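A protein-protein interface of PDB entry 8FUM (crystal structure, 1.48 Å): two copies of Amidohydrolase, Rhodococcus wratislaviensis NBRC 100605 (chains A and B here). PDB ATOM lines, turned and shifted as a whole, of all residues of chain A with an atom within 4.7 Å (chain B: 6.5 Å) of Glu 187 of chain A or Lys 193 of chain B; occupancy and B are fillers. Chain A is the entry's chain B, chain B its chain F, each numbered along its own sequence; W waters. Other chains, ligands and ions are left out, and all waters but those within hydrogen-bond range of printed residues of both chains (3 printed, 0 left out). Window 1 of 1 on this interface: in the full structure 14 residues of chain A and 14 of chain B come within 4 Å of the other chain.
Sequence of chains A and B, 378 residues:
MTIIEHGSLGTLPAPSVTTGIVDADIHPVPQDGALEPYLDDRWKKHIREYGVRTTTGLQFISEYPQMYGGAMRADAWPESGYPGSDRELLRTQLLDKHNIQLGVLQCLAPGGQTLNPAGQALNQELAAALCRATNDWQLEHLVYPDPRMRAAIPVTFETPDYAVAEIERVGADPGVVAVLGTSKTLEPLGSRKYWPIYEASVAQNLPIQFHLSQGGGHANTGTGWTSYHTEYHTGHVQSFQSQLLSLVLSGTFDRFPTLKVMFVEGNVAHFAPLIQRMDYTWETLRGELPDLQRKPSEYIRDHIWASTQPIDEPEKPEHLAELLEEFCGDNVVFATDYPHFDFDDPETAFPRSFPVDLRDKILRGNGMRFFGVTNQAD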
ATOM      1  N   THR A 185     -29.057 -17.761  20.701  1.00  0.00           N
ATOM      2  CA  THR A 185     -28.691 -17.485  19.319  1.00  0.00           C
ATOM      3  C   THR A 185     -28.868 -18.774  18.525  1.00  0.00           C
ATOM      4  O   THR A 185     -29.012 -19.866  19.086  1.00  0.00           O
ATOM      5  CB  THR A 185     -27.243 -17.004  19.194  1.00  0.00           C
ATOM      6  OG1 THR A 185     -26.381 -17.916  19.875  1.00  0.00           O
ATOM      7  CG2 THR A 185     -27.072 -15.617  19.758  1.00  0.00           C
ATOM      8  N   LEU A 186     -28.834 -18.642  17.189  1.00  0.00           N
ATOM      9  CA  LEU A 186     -29.048 -19.802  16.325  1.00  0.00           C
ATOM     10  C   LEU A 186     -27.792 -20.653  16.206  1.00  0.00           C
ATOM     11  O   LEU A 186     -27.881 -21.880  16.016  1.00  0.00           O
ATOM     12  CB  LEU A 186     -29.466 -19.346  14.924  1.00  0.00           C
ATOM     13  CG  LEU A 186     -30.042 -20.402  13.965  1.00  0.00           C
ATOM     14  CD1 LEU A 186     -31.333 -21.009  14.453  1.00  0.00           C
ATOM     15  CD2 LEU A 186     -30.236 -19.775  12.579  1.00  0.00           C
ATOM     16  N   GLU A 187     -26.629 -20.031  16.287  1.00  0.00           N
ATOM     17  CA  GLU A 187     -25.339 -20.682  16.330  1.00  0.00           C
ATOM     18  C   GLU A 187     -24.673 -20.263  17.630  1.00  0.00           C
ATOM     19  O   GLU A 187     -24.868 -19.121  18.072  1.00  0.00           O
ATOM     20  CB  GLU A 187     -24.459 -20.204  15.157  1.00  0.00           C
ATOM     21  CG  GLU A 187     -25.043 -20.539  13.772  1.00  0.00           C
ATOM     22  CD  GLU A 187     -24.183 -20.055  12.600  1.00  0.00           C
ATOM     23  OE1 GLU A 187     -22.961 -20.269  12.647  1.00  0.00           O
ATOM     24  OE2 GLU A 187     -24.749 -19.481  11.636  1.00  0.00           O
ATOM     25  N   PRO A 188     -23.882 -21.123  18.260  1.00  0.00           N
ATOM     26  CA  PRO A 188     -23.185 -20.690  19.475  1.00  0.00           C
ATOM     27  C   PRO A 188     -22.284 -19.503  19.155  1.00  0.00           C
ATOM     28  O   PRO A 188     -21.764 -19.361  18.046  1.00  0.00           O
ATOM     29  CB  PRO A 188     -22.398 -21.931  19.901  1.00  0.00           C
ATOM     30  CG  PRO A 188     -23.237 -23.087  19.348  1.00  0.00           C
ATOM     31  CD  PRO A 188     -23.691 -22.576  18.018  1.00  0.00           C
ATOM     32  N   LEU A 189     -22.105 -18.640  20.155  1.00  0.00           N
ATOM     33  CA  LEU A 189     -21.536 -17.319  19.910  1.00  0.00           C
ATOM     34  C   LEU A 189     -20.065 -17.353  19.495  1.00  0.00           C
ATOM     35  O   LEU A 189     -19.570 -16.347  18.986  1.00  0.00           O
ATOM     36  CB  LEU A 189     -21.725 -16.436  21.154  1.00  0.00           C
ATOM     37  CG  LEU A 189     -23.124 -15.819  21.295  1.00  0.00           C
ATOM     38  CD1 LEU A 189     -23.345 -15.294  22.692  1.00  0.00           C
ATOM     39  CD2 LEU A 189     -23.364 -14.700  20.289  1.00  0.00           C
ATOM     40  N   SER A 191     -19.129 -18.989  16.984  1.00  0.00           N
ATOM     41  CA  SER A 191     -19.187 -19.194  15.545  1.00  0.00           C
ATOM     42  C   SER A 191     -18.668 -17.972  14.797  1.00  0.00           C
ATOM     43  O   SER A 191     -18.873 -16.833  15.201  1.00  0.00           O
ATOM     44  CB  SER A 191     -20.628 -19.466  15.127  1.00  0.00           C
ATOM     45  OG  SER A 191     -21.111 -20.637  15.769  1.00  0.00           O
ATOM     46  N   LYS A 193     -19.820 -16.616  12.317  1.00  0.00           N
ATOM     47  CA  LYS A 193     -20.904 -15.707  11.963  1.00  0.00           C
ATOM     48  C   LYS A 193     -20.792 -14.380  12.691  1.00  0.00           C
ATOM     49  O   LYS A 193     -21.028 -13.315  12.103  1.00  0.00           O
ATOM     50  CB  LYS A 193     -22.260 -16.338  12.315  1.00  0.00           C
ATOM     51  CG  LYS A 193     -23.411 -15.352  12.231  1.00  0.00           C
ATOM     52  CD  LYS A 193     -24.765 -16.054  12.220  1.00  0.00           C
ATOM     53  CE  LYS A 193     -25.854 -15.002  12.098  1.00  0.00           C
ATOM     54  NZ  LYS A 193     -27.214 -15.537  11.921  1.00  0.00           N
ATOM     55  N   TYR A 194     -20.503 -14.439  13.995  1.00  0.00           N
ATOM     56  CA  TYR A 194     -20.589 -13.261  14.846  1.00  0.00           C
ATOM     57  C   TYR A 194     -19.297 -12.464  14.861  1.00  0.00           C
ATOM     58  O   TYR A 194     -19.278 -11.365  15.415  1.00  0.00           O
ATOM     59  CB  TYR A 194     -21.038 -13.667  16.263  1.00  0.00           C
ATOM     60  CG  TYR A 194     -22.324 -14.475  16.220  1.00  0.00           C
ATOM     61  CD1 TYR A 194     -23.522 -13.884  15.862  1.00  0.00           C
ATOM     62  CD2 TYR A 194     -22.332 -15.834  16.530  1.00  0.00           C
ATOM     63  CE1 TYR A 194     -24.705 -14.624  15.786  1.00  0.00           C
ATOM     64  CE2 TYR A 194     -23.506 -16.573  16.469  1.00  0.00           C
ATOM     65  CZ  TYR A 194     -24.668 -15.978  16.094  1.00  0.00           C
ATOM     66  OH  TYR A 194     -25.799 -16.751  16.033  1.00  0.00           O
ATOM     67  N   PHE B 157     -21.396 -23.825   2.824  1.00  0.00           N
ATOM     68  CA  PHE B 157     -22.438 -22.807   2.867  1.00  0.00           C
ATOM     69  C   PHE B 157     -22.615 -22.231   4.252  1.00  0.00           C
ATOM     70  O   PHE B 157     -22.989 -21.056   4.385  1.00  0.00           O
ATOM     71  CB  PHE B 157     -23.770 -23.329   2.314  1.00  0.00           C
ATOM     72  CG  PHE B 157     -23.881 -23.127   0.836  1.00  0.00           C
ATOM     73  CD1 PHE B 157     -23.179 -23.940  -0.043  1.00  0.00           C
ATOM     74  CD2 PHE B 157     -24.576 -22.042   0.308  1.00  0.00           C
ATOM     75  CE1 PHE B 157     -23.226 -23.707  -1.406  1.00  0.00           C
ATOM     76  CE2 PHE B 157     -24.617 -21.818  -1.064  1.00  0.00           C
ATOM     77  CZ  PHE B 157     -23.920 -22.648  -1.903  1.00  0.00           C
ATOM     78  N   GLU B 158     -22.320 -23.010   5.296  1.00  0.00           N
ATOM     79  CA  GLU B 158     -22.521 -22.506   6.645  1.00  0.00           C
ATOM     80  C   GLU B 158     -21.371 -21.636   7.132  1.00  0.00           C
ATOM     81  O   GLU B 158     -21.503 -21.018   8.190  1.00  0.00           O
ATOM     82  CB  GLU B 158     -22.838 -23.636   7.630  1.00  0.00           C
ATOM     83  CG  GLU B 158     -24.045 -24.477   7.255  1.00  0.00           C
ATOM     84  CD  GLU B 158     -25.380 -23.722   7.234  1.00  0.00           C
ATOM     85  OE1 GLU B 158     -25.463 -22.471   7.259  1.00  0.00           O
ATOM     86  OE2 GLU B 158     -26.404 -24.429   7.148  1.00  0.00           O
ATOM     87  N   THR B 159     -20.266 -21.557   6.386  1.00  0.00           N
ATOM     88  CA  THR B 159     -19.215 -20.564   6.646  1.00  0.00           C
ATOM     89  C   THR B 159     -18.903 -19.829   5.345  1.00  0.00           C
ATOM     90  O   THR B 159     -17.972 -20.190   4.601  1.00  0.00           O
ATOM     91  CB  THR B 159     -17.974 -21.182   7.284  1.00  0.00           C
ATOM     92  OG1 THR B 159     -18.357 -21.969   8.414  1.00  0.00           O
ATOM     93  CG2 THR B 159     -17.045 -20.082   7.813  1.00  0.00           C
ATOM     94  N   PRO B 160     -19.662 -18.773   5.045  1.00  0.00           N
ATOM     95  CA  PRO B 160     -19.493 -18.079   3.751  1.00  0.00           C
ATOM     96  C   PRO B 160     -18.092 -17.580   3.480  1.00  0.00           C
ATOM     97  O   PRO B 160     -17.664 -17.607   2.326  1.00  0.00           O
ATOM     98  CB  PRO B 160     -20.523 -16.948   3.832  1.00  0.00           C
ATOM     99  CG  PRO B 160     -21.596 -17.530   4.715  1.00  0.00           C
ATOM    100  CD  PRO B 160     -20.878 -18.328   5.733  1.00  0.00           C
ATOM    101  N   LEU B 186     -29.096 -24.350   8.019  1.00  0.00           N
ATOM    102  CA  LEU B 186     -29.534 -23.907   9.341  1.00  0.00           C
ATOM    103  C   LEU B 186     -30.504 -22.725   9.255  1.00  0.00           C
ATOM    104  O   LEU B 186     -31.384 -22.559  10.119  1.00  0.00           O
ATOM    105  CB  LEU B 186     -28.301 -23.529  10.152  1.00  0.00           C
ATOM    106  CG  LEU B 186     -28.542 -23.303  11.637  1.00  0.00           C
ATOM    107  CD1 LEU B 186     -28.816 -24.616  12.315  1.00  0.00           C
ATOM    108  CD2 LEU B 186     -27.364 -22.612  12.243  1.00  0.00           C
ATOM    109  N   GLU B 187     -30.372 -21.916   8.206  1.00  0.00           N
ATOM    110  CA  GLU B 187     -31.286 -20.849   7.852  1.00  0.00           C
ATOM    111  C   GLU B 187     -31.755 -21.081   6.424  1.00  0.00           C
ATOM    112  O   GLU B 187     -30.984 -21.601   5.611  1.00  0.00           O
ATOM    113  CB  GLU B 187     -30.589 -19.474   7.897  1.00  0.00           C
ATOM    114  CG  GLU B 187     -30.088 -19.075   9.267  1.00  0.00           C
ATOM    115  CD  GLU B 187     -29.395 -17.718   9.251  1.00  0.00           C
ATOM    116  OE1 GLU B 187     -30.025 -16.749   8.804  1.00  0.00           O
ATOM    117  OE2 GLU B 187     -28.235 -17.663   9.685  1.00  0.00           O
ATOM    118  N   GLY B 190     -32.577 -18.056   1.380  1.00  0.00           N
ATOM    119  CA  GLY B 190     -32.748 -16.648   1.066  1.00  0.00           C
ATOM    120  C   GLY B 190     -32.180 -15.716   2.097  1.00  0.00           C
ATOM    121  O   GLY B 190     -32.138 -14.509   1.861  1.00  0.00           O
ATOM    122  N   SER B 191     -31.730 -16.257   3.227  1.00  0.00           N
ATOM    123  CA  SER B 191     -31.144 -15.457   4.289  1.00  0.00           C
ATOM    124  C   SER B 191     -29.906 -14.722   3.799  1.00  0.00           C
ATOM    125  O   SER B 191     -29.105 -15.239   3.014  1.00  0.00           O
ATOM    126  CB  SER B 191     -30.682 -16.373   5.418  1.00  0.00           C
ATOM    127  OG  SER B 191     -29.835 -15.642   6.302  1.00  0.00           O
ATOM    128  N   ARG B 192     -29.717 -13.514   4.339  1.00  0.00           N
ATOM    129  CA  ARG B 192     -28.546 -12.720   3.986  1.00  0.00           C
ATOM    130  C   ARG B 192     -27.236 -13.435   4.310  1.00  0.00           C
ATOM    131  O   ARG B 192     -26.196 -13.110   3.721  1.00  0.00           O
ATOM    132  CB  ARG B 192     -28.631 -11.374   4.705  1.00  0.00           C
ATOM    133  CG  ARG B 192     -27.623 -10.347   4.234  1.00  0.00           C
ATOM    134  CD  ARG B 192     -27.741  -9.038   4.990  1.00  0.00           C
ATOM    135  NE  ARG B 192     -26.741  -8.073   4.535  1.00  0.00           N
ATOM    136  CZ  ARG B 192     -26.951  -7.169   3.578  1.00  0.00           C
ATOM    137  NH1 ARG B 192     -28.126  -7.091   2.954  1.00  0.00           N
ATOM    138  NH2 ARG B 192     -25.969  -6.343   3.247  1.00  0.00           N
ATOM    139  N   LYS B 193     -27.252 -14.402   5.225  1.00  0.00           N
ATOM    140  CA  LYS B 193     -26.028 -15.134   5.513  1.00  0.00           C
ATOM    141  C   LYS B 193     -25.366 -15.644   4.244  1.00  0.00           C
ATOM    142  O   LYS B 193     -24.132 -15.623   4.114  1.00  0.00           O
ATOM    143  CB  LYS B 193     -26.326 -16.311   6.443  1.00  0.00           C
ATOM    144  CG  LYS B 193     -25.155 -17.266   6.573  1.00  0.00           C
ATOM    145  CD  LYS B 193     -25.391 -18.324   7.650  1.00  0.00           C
ATOM    146  CE  LYS B 193     -24.241 -19.319   7.627  1.00  0.00           C
ATOM    147  NZ  LYS B 193     -24.228 -20.269   8.760  1.00  0.00           N
ATOM    148  N   TYR B 194     -26.167 -16.133   3.298  1.00  0.00           N
ATOM    149  CA  TYR B 194     -25.618 -16.812   2.142  1.00  0.00           C
ATOM    150  C   TYR B 194     -25.307 -15.873   1.001  1.00  0.00           C
ATOM    151  O   TYR B 194     -24.651 -16.297   0.043  1.00  0.00           O
ATOM    152  CB  TYR B 194     -26.569 -17.917   1.685  1.00  0.00           C
ATOM    153  CG  TYR B 194     -26.880 -18.870   2.832  1.00  0.00           C
ATOM    154  CD1 TYR B 194     -25.884 -19.652   3.414  1.00  0.00           C
ATOM    155  CD2 TYR B 194     -28.163 -18.930   3.376  1.00  0.00           C
ATOM    156  CE1 TYR B 194     -26.161 -20.485   4.529  1.00  0.00           C
ATOM    157  CE2 TYR B 194     -28.463 -19.772   4.467  1.00  0.00           C
ATOM    158  CZ  TYR B 194     -27.463 -20.553   5.025  1.00  0.00           C
ATOM    159  OH  TYR B 194     -27.753 -21.366   6.120  1.00  0.00           O
ATOM    160  N   TRP B 195     -25.732 -14.617   1.107  1.00  0.00           N
ATOM    161  CA  TRP B 195     -25.517 -13.651   0.034  1.00  0.00           C
ATOM    162  C   TRP B 195     -24.060 -13.483  -0.390  1.00  0.00           C
ATOM    163  O   TRP B 195     -23.814 -13.364  -1.608  1.00  0.00           O
ATOM    164  CB  TRP B 195     -26.195 -12.319   0.396  1.00  0.00           C
ATOM    165  CG  TRP B 195     -27.683 -12.352   0.308  1.00  0.00           C
ATOM    166  CD1 TRP B 195     -28.494 -13.473   0.330  1.00  0.00           C
ATOM    167  CD2 TRP B 195     -28.549 -11.237   0.181  1.00  0.00           C
ATOM    168  NE1 TRP B 195     -29.806 -13.100   0.227  1.00  0.00           N
ATOM    169  CE2 TRP B 195     -29.865 -11.734   0.120  1.00  0.00           C
ATOM    170  CE3 TRP B 195     -28.340  -9.850   0.093  1.00  0.00           C
ATOM    171  CZ2 TRP B 195     -30.966 -10.903  -0.010  1.00  0.00           C
ATOM    172  CZ3 TRP B 195     -29.457  -9.023  -0.026  1.00  0.00           C
ATOM    173  CH2 TRP B 195     -30.740  -9.557  -0.096  1.00  0.00           C
ATOM    174  N   PRO B 196     -23.059 -13.502   0.498  1.00  0.00           N
ATOM    175  CA  PRO B 196     -21.679 -13.421  -0.010  1.00  0.00           C
ATOM    176  C   PRO B 196     -21.288 -14.578  -0.917  1.00  0.00           C
ATOM    177  O   PRO B 196     -20.457 -14.399  -1.819  1.00  0.00           O
ATOM    178  CB  PRO B 196     -20.825 -13.359   1.266  1.00  0.00           C
ATOM    179  CG  PRO B 196     -21.758 -12.892   2.323  1.00  0.00           C
ATOM    180  CD  PRO B 196     -23.096 -13.460   1.970  1.00  0.00           C
ATOM    181  N   ILE B 197     -21.891 -15.758  -0.727  1.00  0.00           N
ATOM    182  CA  ILE B 197     -21.636 -16.883  -1.617  1.00  0.00           C
ATOM    183  C   ILE B 197     -22.275 -16.642  -2.971  1.00  0.00           C
ATOM    184  O   ILE B 197     -21.666 -16.913  -4.016  1.00  0.00           O
ATOM    185  CB  ILE B 197     -22.139 -18.200  -0.983  1.00  0.00           C
ATOM    186  CG1 ILE B 197     -21.421 -18.446   0.337  1.00  0.00           C
ATOM    187  CG2 ILE B 197     -21.950 -19.357  -1.974  1.00  0.00           C
ATOM    188  CD1 ILE B 197     -21.946 -19.627   1.129  1.00  0.00           C
HETATM  189  O   HOH W   1     -21.742 -22.537  10.832  1.00  0.00           O
HETATM  190  O   HOH W   2     -30.176 -16.225  12.126  1.00  0.00           O
HETATM  191  O   HOH W   3     -27.650 -15.034   9.399  1.00  0.00           O
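NZ of Lys 193 of chain B is in salt-bridge range of OE2 of Glu 187 of chain A, 3.0 Å away. NZ of Lys 193 of chain A lies within salt-bridge range of OE2 of Glu 187 of chain B, 3.2 Å away.
The side-chain hydroxyl of Ser 191 of chain B lies within hydrogen-bond range of the side-chain carboxylate of Glu 187 of chain B (2.7 Å). N of Lys 193 of chain B sits close to OG of Ser 191 of chain B, 3.1 Å away. The backbone carbonyl oxygen (O) of Glu 187 of chain B is in hydrogen-bond range of the side-chain hydroxyl (OH) of Tyr 194 of chain B (3.3 Å). N of Leu 186 of chain B lies within hydrogen-bond range of OE2 of Glu 158 of chain B (2.8 Å). O of Glu 187 of chain A lies within hydrogen-bond range of OH of Tyr 194 of chain A (3.3 Å). OE1 of Glu 158 of chain B lies within salt-bridge range of NZ of Lys 193 of chain B.
CG of Leu 186 of chain A touches CD2 of Leu 186 of chain B, at 3.9 Å. CD2 of Leu 186 of chain A touches CG of Glu 187 of chain B, 3.4 Å away. CD2 of Leu 186 of chain B touches CG of Glu 187 of chain A (3.5 Å).
Of the printed residues of chain B, Glu 187 of chain A touches Leu 186 and Lys 193. Printed residues of chain A within 4 Å of Glu 187 of chain B: Leu 186 (3.4 Å) and Lys 193 (3.2 Å). Printed residues of chain B within 4 Å of Leu 186 of chain A: Leu 186 and Glu 187. Printed residues of chain A within 4 Å of Leu 186 of chain B: Leu 186 and Glu 187. Of the printed residues of chain B, Lys 193 of chain A touches Glu 187 (3.2 Å). The nearest residue of chain B that does not touch Glu 187 of chain A is Glu 187 of chain B (4.4 Å). The nearest printed residue of chain A that does not touch Leu 186 of chain B is Pro 188 of chain A (6.8 Å).
Of the 14 printed residues of chain B, 3 touch a printed residue of chain A. Printed residues of chain B that touch a printed residue of chain A: Leu 186, Glu 187 and Lys 193. Among the printed residues, 5 pairs touch across the chains. Among the printed residues, Asp or Glu carboxylates within 4 Å of a Lys or Arg side-chain nitrogen of the other chain: Glu 187 of chain A with Lys 193 of chain B and Lys 193 of chain A with Glu 187 of chain B.
Leu 186 of chain B touches its own counterpart, Leu 186 of chain A. Leu 186 of chain A touches Glu 187 of chain B, and with the chains exchanged Glu 187 of chain A touches Leu 186 of chain B. Glu 187 of chain A touches Lys 193 of chain B, and with the chains exchanged Lys 193 of chain A touches Glu 187 of chain B. Positions printed for both chains: 186, 187, 191, 193 and 194. Of the 5 pairs that touch across the chains among the printed residues, 5 have their exchanged pair printed and touching as well.
Water W3 bridges the side-chain amino group of Lys 193 of chain A (2.6 Å) and the side-chain carboxylate of Glu 187 of chain B (2.7 Å). Water W2 lies within hydrogen-bond range of NZ of Lys 193 of chain A and OE1 of Glu 187 of chain B. Water W1 lies within hydrogen-bond range of the backbone carbonyl oxygen (O) of Glu 158 of chain B (3.1 Å) and the side-chain carboxylate (OE1) of Glu 187 of chain A (3.2 Å).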
